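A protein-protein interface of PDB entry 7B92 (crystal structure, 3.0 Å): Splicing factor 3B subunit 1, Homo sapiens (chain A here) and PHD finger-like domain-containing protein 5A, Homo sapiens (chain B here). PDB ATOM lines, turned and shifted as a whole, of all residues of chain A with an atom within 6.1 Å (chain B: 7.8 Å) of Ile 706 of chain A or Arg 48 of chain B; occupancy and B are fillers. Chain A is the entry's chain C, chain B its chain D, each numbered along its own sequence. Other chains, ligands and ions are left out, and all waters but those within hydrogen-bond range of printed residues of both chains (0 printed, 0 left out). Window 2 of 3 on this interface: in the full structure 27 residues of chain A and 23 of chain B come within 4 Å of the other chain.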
ATOM      1  N   ALA A 665      -0.611  32.353  -1.491  1.00  0.00           N
ATOM      2  CA  ALA A 665      -0.696  32.773  -2.888  1.00  0.00           C
ATOM      3  C   ALA A 665      -2.062  33.368  -3.214  1.00  0.00           C
ATOM      4  O   ALA A 665      -2.158  34.333  -3.982  1.00  0.00           O
ATOM      5  CB  ALA A 665      -0.394  31.595  -3.810  1.00  0.00           C
ATOM      6  N   ALA A 668      -2.037  36.804  -1.924  1.00  0.00           N
ATOM      7  CA  ALA A 668      -1.167  37.631  -2.756  1.00  0.00           C
ATOM      8  C   ALA A 668      -1.812  37.977  -4.089  1.00  0.00           C
ATOM      9  O   ALA A 668      -1.479  39.004  -4.689  1.00  0.00           O
ATOM     10  CB  ALA A 668       0.162  36.919  -2.999  1.00  0.00           C
ATOM     11  N   GLU A 669      -2.704  37.124  -4.586  1.00  0.00           N
ATOM     12  CA  GLU A 669      -3.375  37.432  -5.841  1.00  0.00           C
ATOM     13  C   GLU A 669      -4.574  38.346  -5.621  1.00  0.00           C
ATOM     14  O   GLU A 669      -4.751  39.320  -6.359  1.00  0.00           O
ATOM     15  CB  GLU A 669      -3.797  36.141  -6.545  1.00  0.00           C
ATOM     16  CG  GLU A 669      -4.078  36.302  -8.035  1.00  0.00           C
ATOM     17  CD  GLU A 669      -5.498  36.752  -8.323  1.00  0.00           C
ATOM     18  OE1 GLU A 669      -6.402  36.432  -7.519  1.00  0.00           O
ATOM     19  OE2 GLU A 669      -5.709  37.429  -9.350  1.00  0.00           O
ATOM     20  N   PRO A 673       0.122  41.917  -4.334  1.00  0.00           N
ATOM     21  CA  PRO A 673       1.226  41.167  -3.701  1.00  0.00           C
ATOM     22  C   PRO A 673       2.177  42.009  -2.861  1.00  0.00           C
ATOM     23  O   PRO A 673       3.018  41.431  -2.160  1.00  0.00           O
ATOM     24  CB  PRO A 673       1.962  40.545  -4.896  1.00  0.00           C
ATOM     25  CG  PRO A 673       0.965  40.533  -6.002  1.00  0.00           C
ATOM     26  CD  PRO A 673       0.118  41.754  -5.797  1.00  0.00           C
ATOM     27  N   PHE A 701       5.331  28.851  -5.457  1.00  0.00           N
ATOM     28  CA  PHE A 701       3.926  28.721  -5.828  1.00  0.00           C
ATOM     29  C   PHE A 701       3.250  30.077  -5.991  1.00  0.00           C
ATOM     30  O   PHE A 701       2.350  30.211  -6.824  1.00  0.00           O
ATOM     31  CB  PHE A 701       3.156  27.880  -4.816  1.00  0.00           C
ATOM     32  CG  PHE A 701       1.718  27.681  -5.193  1.00  0.00           C
ATOM     33  CD1 PHE A 701       1.374  26.810  -6.211  1.00  0.00           C
ATOM     34  CD2 PHE A 701       0.713  28.385  -4.554  1.00  0.00           C
ATOM     35  CE1 PHE A 701       0.055  26.637  -6.577  1.00  0.00           C
ATOM     36  CE2 PHE A 701      -0.610  28.213  -4.916  1.00  0.00           C
ATOM     37  CZ  PHE A 701      -0.938  27.338  -5.927  1.00  0.00           C
ATOM     38  N   LEU A 702       3.673  31.091  -5.232  1.00  0.00           N
ATOM     39  CA  LEU A 702       3.072  32.415  -5.348  1.00  0.00           C
ATOM     40  C   LEU A 702       3.294  32.995  -6.736  1.00  0.00           C
ATOM     41  O   LEU A 702       2.364  33.524  -7.361  1.00  0.00           O
ATOM     42  CB  LEU A 702       3.652  33.337  -4.273  1.00  0.00           C
ATOM     43  CG  LEU A 702       3.041  34.722  -4.036  1.00  0.00           C
ATOM     44  CD1 LEU A 702       3.241  35.116  -2.589  1.00  0.00           C
ATOM     45  CD2 LEU A 702       3.671  35.764  -4.938  1.00  0.00           C
ATOM     46  N   PHE A 703       4.529  32.913  -7.230  1.00  0.00           N
ATOM     47  CA  PHE A 703       4.806  33.449  -8.557  1.00  0.00           C
ATOM     48  C   PHE A 703       4.145  32.609  -9.637  1.00  0.00           C
ATOM     49  O   PHE A 703       3.603  33.157 -10.608  1.00  0.00           O
ATOM     50  CB  PHE A 703       6.311  33.561  -8.782  1.00  0.00           C
ATOM     51  CG  PHE A 703       6.904  34.804  -8.193  1.00  0.00           C
ATOM     52  CD1 PHE A 703       6.905  35.988  -8.909  1.00  0.00           C
ATOM     53  CD2 PHE A 703       7.436  34.796  -6.916  1.00  0.00           C
ATOM     54  CE1 PHE A 703       7.435  37.139  -8.368  1.00  0.00           C
ATOM     55  CE2 PHE A 703       7.968  35.942  -6.368  1.00  0.00           C
ATOM     56  CZ  PHE A 703       7.967  37.118  -7.096  1.00  0.00           C
ATOM     57  N   GLU A 704       4.137  31.281  -9.475  1.00  0.00           N
ATOM     58  CA  GLU A 704       3.434  30.455 -10.452  1.00  0.00           C
ATOM     59  C   GLU A 704       1.948  30.789 -10.498  1.00  0.00           C
ATOM     60  O   GLU A 704       1.338  30.764 -11.573  1.00  0.00           O
ATOM     61  CB  GLU A 704       3.643  28.970 -10.146  1.00  0.00           C
ATOM     62  CG  GLU A 704       3.030  28.032 -11.186  1.00  0.00           C
ATOM     63  CD  GLU A 704       3.360  26.573 -10.932  1.00  0.00           C
ATOM     64  OE1 GLU A 704       3.868  26.256  -9.837  1.00  0.00           O
ATOM     65  OE2 GLU A 704       3.114  25.743 -11.832  1.00  0.00           O
ATOM     66  N   TYR A 705       1.357  31.134  -9.353  1.00  0.00           N
ATOM     67  CA  TYR A 705      -0.075  31.398  -9.300  1.00  0.00           C
ATOM     68  C   TYR A 705      -0.423  32.772  -9.858  1.00  0.00           C
ATOM     69  O   TYR A 705      -1.389  32.904 -10.618  1.00  0.00           O
ATOM     70  CB  TYR A 705      -0.575  31.257  -7.859  1.00  0.00           C
ATOM     71  CG  TYR A 705      -2.072  31.364  -7.718  1.00  0.00           C
ATOM     72  CD1 TYR A 705      -2.899  30.307  -8.073  1.00  0.00           C
ATOM     73  CD2 TYR A 705      -2.660  32.516  -7.217  1.00  0.00           C
ATOM     74  CE1 TYR A 705      -4.271  30.401  -7.946  1.00  0.00           C
ATOM     75  CE2 TYR A 705      -4.032  32.618  -7.083  1.00  0.00           C
ATOM     76  CZ  TYR A 705      -4.833  31.559  -7.449  1.00  0.00           C
ATOM     77  OH  TYR A 705      -6.198  31.658  -7.318  1.00  0.00           O
ATOM     78  N   ILE A 706       0.348  33.805  -9.503  1.00  0.00           N
ATOM     79  CA  ILE A 706       0.035  35.153  -9.980  1.00  0.00           C
ATOM     80  C   ILE A 706       0.425  35.365 -11.433  1.00  0.00           C
ATOM     81  O   ILE A 706      -0.181  36.209 -12.110  1.00  0.00           O
ATOM     82  CB  ILE A 706       0.700  36.234  -9.115  1.00  0.00           C
ATOM     83  CG1 ILE A 706       2.226  36.111  -9.155  1.00  0.00           C
ATOM     84  CG2 ILE A 706       0.188  36.169  -7.692  1.00  0.00           C
ATOM     85  CD1 ILE A 706       2.928  37.090  -8.260  1.00  0.00           C
ATOM     86  N   GLY A 707       1.407  34.626 -11.946  1.00  0.00           N
ATOM     87  CA  GLY A 707       1.651  34.693 -13.372  1.00  0.00           C
ATOM     88  C   GLY A 707       2.182  36.067 -13.743  1.00  0.00           C
ATOM     89  O   GLY A 707       3.211  36.528 -13.230  1.00  0.00           O
ATOM     90  N   GLU A 708       1.472  36.742 -14.646  1.00  0.00           N
ATOM     91  CA  GLU A 708       1.923  38.038 -15.138  1.00  0.00           C
ATOM     92  C   GLU A 708       1.851  39.122 -14.072  1.00  0.00           C
ATOM     93  O   GLU A 708       2.490  40.169 -14.224  1.00  0.00           O
ATOM     94  CB  GLU A 708       1.097  38.450 -16.359  1.00  0.00           C
ATOM     95  CG  GLU A 708      -0.340  38.856 -16.052  1.00  0.00           C
ATOM     96  CD  GLU A 708      -0.515  40.364 -15.906  1.00  0.00           C
ATOM     97  OE1 GLU A 708       0.480  41.103 -16.067  1.00  0.00           O
ATOM     98  OE2 GLU A 708      -1.654  40.814 -15.653  1.00  0.00           O
ATOM     99  N   MET A 709       1.086  38.895 -13.002  1.00  0.00           N
ATOM    100  CA  MET A 709       0.962  39.897 -11.950  1.00  0.00           C
ATOM    101  C   MET A 709       2.292  40.146 -11.255  1.00  0.00           C
ATOM    102  O   MET A 709       2.531  41.249 -10.749  1.00  0.00           O
ATOM    103  CB  MET A 709      -0.097  39.455 -10.940  1.00  0.00           C
ATOM    104  CG  MET A 709      -0.598  40.554 -10.029  1.00  0.00           C
ATOM    105  SD  MET A 709      -1.887  39.966  -8.916  1.00  0.00           S
ATOM    106  CE  MET A 709      -2.489  41.519  -8.253  1.00  0.00           C
ATOM    107  N   GLY A 710       3.171  39.148 -11.228  1.00  0.00           N
ATOM    108  CA  GLY A 710       4.475  39.274 -10.617  1.00  0.00           C
ATOM    109  C   GLY A 710       5.498  40.046 -11.415  1.00  0.00           C
ATOM    110  O   GLY A 710       6.680  40.026 -11.062  1.00  0.00           O
ATOM    111  N   LYS A 711       5.081  40.727 -12.487  1.00  0.00           N
ATOM    112  CA  LYS A 711       6.007  41.517 -13.288  1.00  0.00           C
ATOM    113  C   LYS A 711       6.592  42.688 -12.512  1.00  0.00           C
ATOM    114  O   LYS A 711       7.666  43.180 -12.870  1.00  0.00           O
ATOM    115  CB  LYS A 711       5.308  42.031 -14.548  1.00  0.00           C
ATOM    116  CG  LYS A 711       4.103  42.919 -14.275  1.00  0.00           C
ATOM    117  CD  LYS A 711       3.382  43.294 -15.563  1.00  0.00           C
ATOM    118  CE  LYS A 711       2.117  44.093 -15.282  1.00  0.00           C
ATOM    119  NZ  LYS A 711       2.398  45.376 -14.575  1.00  0.00           N
ATOM    120  N   TYR A 713       7.537  42.559  -9.302  1.00  0.00           N
ATOM    121  CA  TYR A 713       8.071  42.031  -8.054  1.00  0.00           C
ATOM    122  C   TYR A 713       9.291  41.133  -8.238  1.00  0.00           C
ATOM    123  O   TYR A 713       9.743  40.531  -7.258  1.00  0.00           O
ATOM    124  CB  TYR A 713       6.986  41.260  -7.296  1.00  0.00           C
ATOM    125  CG  TYR A 713       5.771  42.088  -6.945  1.00  0.00           C
ATOM    126  CD1 TYR A 713       5.763  42.906  -5.823  1.00  0.00           C
ATOM    127  CD2 TYR A 713       4.632  42.055  -7.739  1.00  0.00           C
ATOM    128  CE1 TYR A 713       4.650  43.666  -5.499  1.00  0.00           C
ATOM    129  CE2 TYR A 713       3.518  42.810  -7.425  1.00  0.00           C
ATOM    130  CZ  TYR A 713       3.531  43.613  -6.304  1.00  0.00           C
ATOM    131  OH  TYR A 713       2.423  44.365  -5.988  1.00  0.00           O
ATOM    132  N   GLY B  38      -7.563  17.916 -11.732  1.00  0.00           N
ATOM    133  CA  GLY B  38      -7.006  19.178 -12.193  1.00  0.00           C
ATOM    134  C   GLY B  38      -5.519  19.145 -12.480  1.00  0.00           C
ATOM    135  O   GLY B  38      -4.993  20.118 -13.030  1.00  0.00           O
ATOM    136  N   CYS B  40      -1.811  18.513 -14.014  1.00  0.00           N
ATOM    137  CA  CYS B  40      -1.242  18.508 -15.352  1.00  0.00           C
ATOM    138  C   CYS B  40      -0.468  17.219 -15.589  1.00  0.00           C
ATOM    139  O   CYS B  40       0.161  16.672 -14.679  1.00  0.00           O
ATOM    140  CB  CYS B  40      -0.325  19.714 -15.557  1.00  0.00           C
ATOM    141  SG  CYS B  40       0.690  19.640 -17.052  1.00  0.00           S
ATOM    142  N   SER B  45       1.303  20.002 -12.046  1.00  0.00           N
ATOM    143  CA  SER B  45       0.800  21.269 -11.539  1.00  0.00           C
ATOM    144  C   SER B  45      -0.716  21.333 -11.665  1.00  0.00           C
ATOM    145  O   SER B  45      -1.312  20.719 -12.553  1.00  0.00           O
ATOM    146  CB  SER B  45       1.418  22.454 -12.284  1.00  0.00           C
ATOM    147  OG  SER B  45       0.781  23.666 -11.913  1.00  0.00           O
ATOM    148  N   TYR B  46      -1.332  22.097 -10.765  1.00  0.00           N
ATOM    149  CA  TYR B  46      -2.773  22.303 -10.761  1.00  0.00           C
ATOM    150  C   TYR B  46      -3.155  23.717 -11.180  1.00  0.00           C
ATOM    151  O   TYR B  46      -4.309  24.117 -10.997  1.00  0.00           O
ATOM    152  CB  TYR B  46      -3.345  21.999  -9.373  1.00  0.00           C
ATOM    153  CG  TYR B  46      -3.255  20.548  -8.961  1.00  0.00           C
ATOM    154  CD1 TYR B  46      -2.091  20.032  -8.404  1.00  0.00           C
ATOM    155  CD2 TYR B  46      -4.337  19.694  -9.118  1.00  0.00           C
ATOM    156  CE1 TYR B  46      -2.008  18.707  -8.021  1.00  0.00           C
ATOM    157  CE2 TYR B  46      -4.263  18.366  -8.737  1.00  0.00           C
ATOM    158  CZ  TYR B  46      -3.097  17.879  -8.191  1.00  0.00           C
ATOM    159  OH  TYR B  46      -3.024  16.559  -7.814  1.00  0.00           O
ATOM    160  N   VAL B  47      -2.219  24.479 -11.742  1.00  0.00           N
ATOM    161  CA  VAL B  47      -2.408  25.902 -12.005  1.00  0.00           C
ATOM    162  C   VAL B  47      -2.682  26.116 -13.486  1.00  0.00           C
ATOM    163  O   VAL B  47      -1.899  25.682 -14.341  1.00  0.00           O
ATOM    164  CB  VAL B  47      -1.181  26.715 -11.561  1.00  0.00           C
ATOM    165  CG1 VAL B  47      -1.537  28.184 -11.449  1.00  0.00           C
ATOM    166  CG2 VAL B  47      -0.650  26.189 -10.241  1.00  0.00           C
ATOM    167  N   ARG B  48      -3.788  26.798 -13.786  1.00  0.00           N
ATOM    168  CA  ARG B  48      -4.137  27.266 -15.122  1.00  0.00           C
ATOM    169  C   ARG B  48      -4.116  26.156 -16.164  1.00  0.00           C
ATOM    170  O   ARG B  48      -3.177  26.081 -16.968  1.00  0.00           O
ATOM    171  CB  ARG B  48      -3.193  28.389 -15.557  1.00  0.00           C
ATOM    172  CG  ARG B  48      -3.417  29.704 -14.835  1.00  0.00           C
ATOM    173  CD  ARG B  48      -2.574  30.813 -15.441  1.00  0.00           C
ATOM    174  NE  ARG B  48      -2.705  32.061 -14.697  1.00  0.00           N
ATOM    175  CZ  ARG B  48      -1.942  32.401 -13.664  1.00  0.00           C
ATOM    176  NH1 ARG B  48      -0.984  31.586 -13.246  1.00  0.00           N
ATOM    177  NH2 ARG B  48      -2.136  33.559 -13.049  1.00  0.00           N
ATOM    178  N   PRO B  49      -5.121  25.283 -16.189  1.00  0.00           N
ATOM    179  CA  PRO B  49      -5.262  24.353 -17.320  1.00  0.00           C
ATOM    180  C   PRO B  49      -5.462  25.127 -18.613  1.00  0.00           C
ATOM    181  O   PRO B  49      -6.383  25.936 -18.737  1.00  0.00           O
ATOM    182  CB  PRO B  49      -6.500  23.529 -16.947  1.00  0.00           C
ATOM    183  CG  PRO B  49      -6.623  23.672 -15.467  1.00  0.00           C
ATOM    184  CD  PRO B  49      -6.145  25.053 -15.156  1.00  0.00           C
ATOM    185  N   CYS B  50      -4.583  24.879 -19.583  1.00  0.00           N
ATOM    186  CA  CYS B  50      -4.563  25.671 -20.803  1.00  0.00           C
ATOM    187  C   CYS B  50      -5.024  24.861 -22.010  1.00  0.00           C
ATOM    188  O   CYS B  50      -6.181  24.975 -22.426  1.00  0.00           O
ATOM    189  CB  CYS B  50      -3.161  26.232 -21.039  1.00  0.00           C
ATOM    190  SG  CYS B  50      -3.100  27.577 -22.230  1.00  0.00           S
ATOM    191  N   THR B  51      -4.138  24.047 -22.580  1.00  0.00           N
ATOM    192  CA  THR B  51      -4.424  23.335 -23.820  1.00  0.00           C
ATOM    193  C   THR B  51      -4.917  21.921 -23.536  1.00  0.00           C
ATOM    194  O   THR B  51      -4.434  21.252 -22.618  1.00  0.00           O
ATOM    195  CB  THR B  51      -3.191  23.272 -24.725  1.00  0.00           C
ATOM    196  OG1 THR B  51      -2.120  22.627 -24.029  1.00  0.00           O
ATOM    197  CG2 THR B  51      -2.755  24.671 -25.136  1.00  0.00           C
ATOM    198  N   TYR B  80      -5.642  18.258 -19.385  1.00  0.00           N
ATOM    199  CA  TYR B  80      -5.114  19.513 -19.902  1.00  0.00           C
ATOM    200  C   TYR B  80      -3.652  19.673 -19.511  1.00  0.00           C
ATOM    201  O   TYR B  80      -3.263  19.354 -18.385  1.00  0.00           O
ATOM    202  CB  TYR B  80      -5.904  20.721 -19.374  1.00  0.00           C
ATOM    203  CG  TYR B  80      -7.308  20.854 -19.919  1.00  0.00           C
ATOM    204  CD1 TYR B  80      -8.368  20.179 -19.330  1.00  0.00           C
ATOM    205  CD2 TYR B  80      -7.575  21.667 -21.014  1.00  0.00           C
ATOM    206  CE1 TYR B  80      -9.654  20.302 -19.819  1.00  0.00           C
ATOM    207  CE2 TYR B  80      -8.860  21.797 -21.512  1.00  0.00           C
ATOM    208  CZ  TYR B  80      -9.895  21.111 -20.910  1.00  0.00           C
ATOM    209  OH  TYR B  80     -11.178  21.229 -21.395  1.00  0.00           O
ATOM    210  N   TYR B  81      -2.847  20.170 -20.447  1.00  0.00           N
ATOM    211  CA  TYR B  81      -1.553  20.727 -20.085  1.00  0.00           C
ATOM    212  C   TYR B  81      -1.760  22.017 -19.297  1.00  0.00           C
ATOM    213  O   TYR B  81      -2.838  22.613 -19.309  1.00  0.00           O
ATOM    214  CB  TYR B  81      -0.711  21.017 -21.329  1.00  0.00           C
ATOM    215  CG  TYR B  81      -0.383  19.808 -22.177  1.00  0.00           C
ATOM    216  CD1 TYR B  81      -1.227  19.408 -23.202  1.00  0.00           C
ATOM    217  CD2 TYR B  81       0.779  19.079 -21.962  1.00  0.00           C
ATOM    218  CE1 TYR B  81      -0.932  18.309 -23.981  1.00  0.00           C
ATOM    219  CE2 TYR B  81       1.082  17.978 -22.739  1.00  0.00           C
ATOM    220  CZ  TYR B  81       0.224  17.597 -23.747  1.00  0.00           C
ATOM    221  OH  TYR B  81       0.519  16.502 -24.527  1.00  0.00           O
ATOM    222  N   CYS B  82      -0.715  22.448 -18.603  1.00  0.00           N
ATOM    223  CA  CYS B  82      -0.795  23.698 -17.865  1.00  0.00           C
ATOM    224  C   CYS B  82      -0.295  24.854 -18.729  1.00  0.00           C
ATOM    225  O   CYS B  82       0.277  24.663 -19.806  1.00  0.00           O
ATOM    226  CB  CYS B  82       0.004  23.608 -16.565  1.00  0.00           C
ATOM    227  SG  CYS B  82       1.785  23.606 -16.805  1.00  0.00           S
ATOM    228  N   LYS B  83      -0.527  26.076 -18.243  1.00  0.00           N
ATOM    229  CA  LYS B  83      -0.095  27.261 -18.978  1.00  0.00           C
ATOM    230  C   LYS B  83       1.419  27.286 -19.149  1.00  0.00           C
ATOM    231  O   LYS B  83       1.925  27.695 -20.202  1.00  0.00           O
ATOM    232  CB  LYS B  83      -0.579  28.524 -18.262  1.00  0.00           C
ATOM    233  CG  LYS B  83      -0.252  29.824 -18.978  1.00  0.00           C
ATOM    234  CD  LYS B  83      -0.898  29.888 -20.349  1.00  0.00           C
ATOM    235  CE  LYS B  83      -0.610  31.217 -21.031  1.00  0.00           C
ATOM    236  NZ  LYS B  83      -1.098  32.372 -20.219  1.00  0.00           N
ATOM    237  N   GLU B  84       2.161  26.850 -18.128  1.00  0.00           N
ATOM    238  CA  GLU B  84       3.618  26.826 -18.220  1.00  0.00           C
ATOM    239  C   GLU B  84       4.088  25.894 -19.331  1.00  0.00           C
ATOM    240  O   GLU B  84       4.969  26.246 -20.124  1.00  0.00           O
ATOM    241  CB  GLU B  84       4.223  26.404 -16.883  1.00  0.00           C
ATOM    242  CG  GLU B  84       4.080  27.424 -15.777  1.00  0.00           C
ATOM    243  CD  GLU B  84       4.889  27.054 -14.549  1.00  0.00           C
ATOM    244  OE1 GLU B  84       5.166  25.849 -14.360  1.00  0.00           O
ATOM    245  OE2 GLU B  84       5.252  27.968 -13.778  1.00  0.00           O
ATOM    246  N   CYS B  85       3.516  24.687 -19.393  1.00  0.00           N
ATOM    247  CA  CYS B  85       3.904  23.743 -20.434  1.00  0.00           C
ATOM    248  C   CYS B  85       3.444  24.205 -21.810  1.00  0.00           C
ATOM    249  O   CYS B  85       4.100  23.906 -22.814  1.00  0.00           O
ATOM    250  CB  CYS B  85       3.354  22.354 -20.114  1.00  0.00           C
ATOM    251  SG  CYS B  85       4.077  21.607 -18.634  1.00  0.00           S
ATOM    252  N   THR B  86       2.327  24.932 -21.881  1.00  0.00           N
ATOM    253  CA  THR B  86       1.915  25.520 -23.151  1.00  0.00           C
ATOM    254  C   THR B  86       2.919  26.566 -23.618  1.00  0.00           C
ATOM    255  O   THR B  86       3.278  26.606 -24.801  1.00  0.00           O
ATOM    256  CB  THR B  86       0.525  26.137 -23.018  1.00  0.00           C
ATOM    257  OG1 THR B  86      -0.420  25.121 -22.665  1.00  0.00           O
ATOM    258  CG2 THR B  86       0.102  26.770 -24.327  1.00  0.00           C
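The side-chain carboxylate (OE2) of Glu 704 of chain A lies within hydrogen-bond range of the side-chain hydroxyl (OG) of Ser 45 of chain B, at 3.1 Å.
The backbone carbonyl oxygen (O) of Glu 704 of chain A is in hydrogen-bond range of the guanidinium group (NH1) of Arg 48 of chain B, 3.0 Å away.
The backbone carbonyl oxygen (O) of Tyr 705 of chain A is in hydrogen-bond range of the guanidinium group (NH2) of Arg 48 of chain B, 2.6 Å away.
O of Ile 706 of chain A is in hydrogen-bond range of NH2 of Arg 48 of chain B (3.4 Å).
The side-chain carboxylate (OE1) of Glu 84 of chain B sits close to the side-chain carboxylate (OE2) of Glu 704 of chain A, 3.3 Å away.
N of Cys 40 of chain B lies within hydrogen-bond range of O of Ser 45 of chain B.
OG of Ser 45 of chain B is in hydrogen-bond range of N of Val 47 of chain B, 3.1 Å away.
The backbone NH of Lys 83 of chain B sits at hydrogen-bond distance from the backbone carbonyl oxygen of Arg 48 of chain B (2.9 Å).
N of Glu 84 of chain B lies close to SG of Cys 82 of chain B, at 3.5 Å.
Among the printed residues, merely in contact across the chains: Phe 701 of chain A with Val 47 of chain B (3.8 Å), Gly 707 of chain A with Arg 48 of chain B (3.9 Å) and Glu 704 of chain A with Val 47 of chain B (3.9 Å).
Of chain B, only Arg 48 comes within 4 Å of Ile 706 of chain A.
Printed residues of chain A within 4 Å of Arg 48 of chain B: Glu 704, Tyr 705, Ile 706 and Gly 707.
Of the printed residues of chain A, Ser 45 of chain B touches Glu 704.
Printed residues of chain A within 4 Å of Val 47 of chain B: Phe 701 and Glu 704.
Tyr 46 of chain B touches none of the printed residues of chain A.
Cys 85 of chain B touches none of the printed residues of chain A.
The nearest printed residue of chain A that does not touch Val 47 of chain B is Tyr 705 of chain A (4.1 Å).
Of the 16 printed residues of chain A, 5 touch a printed residue of chain B.
Hydrophobic or aromatic side chains of chain A that line the printed part of chain B: Phe 701.
Along chain A the printed residues that touch a printed residue of chain B span positions 701 to 707.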
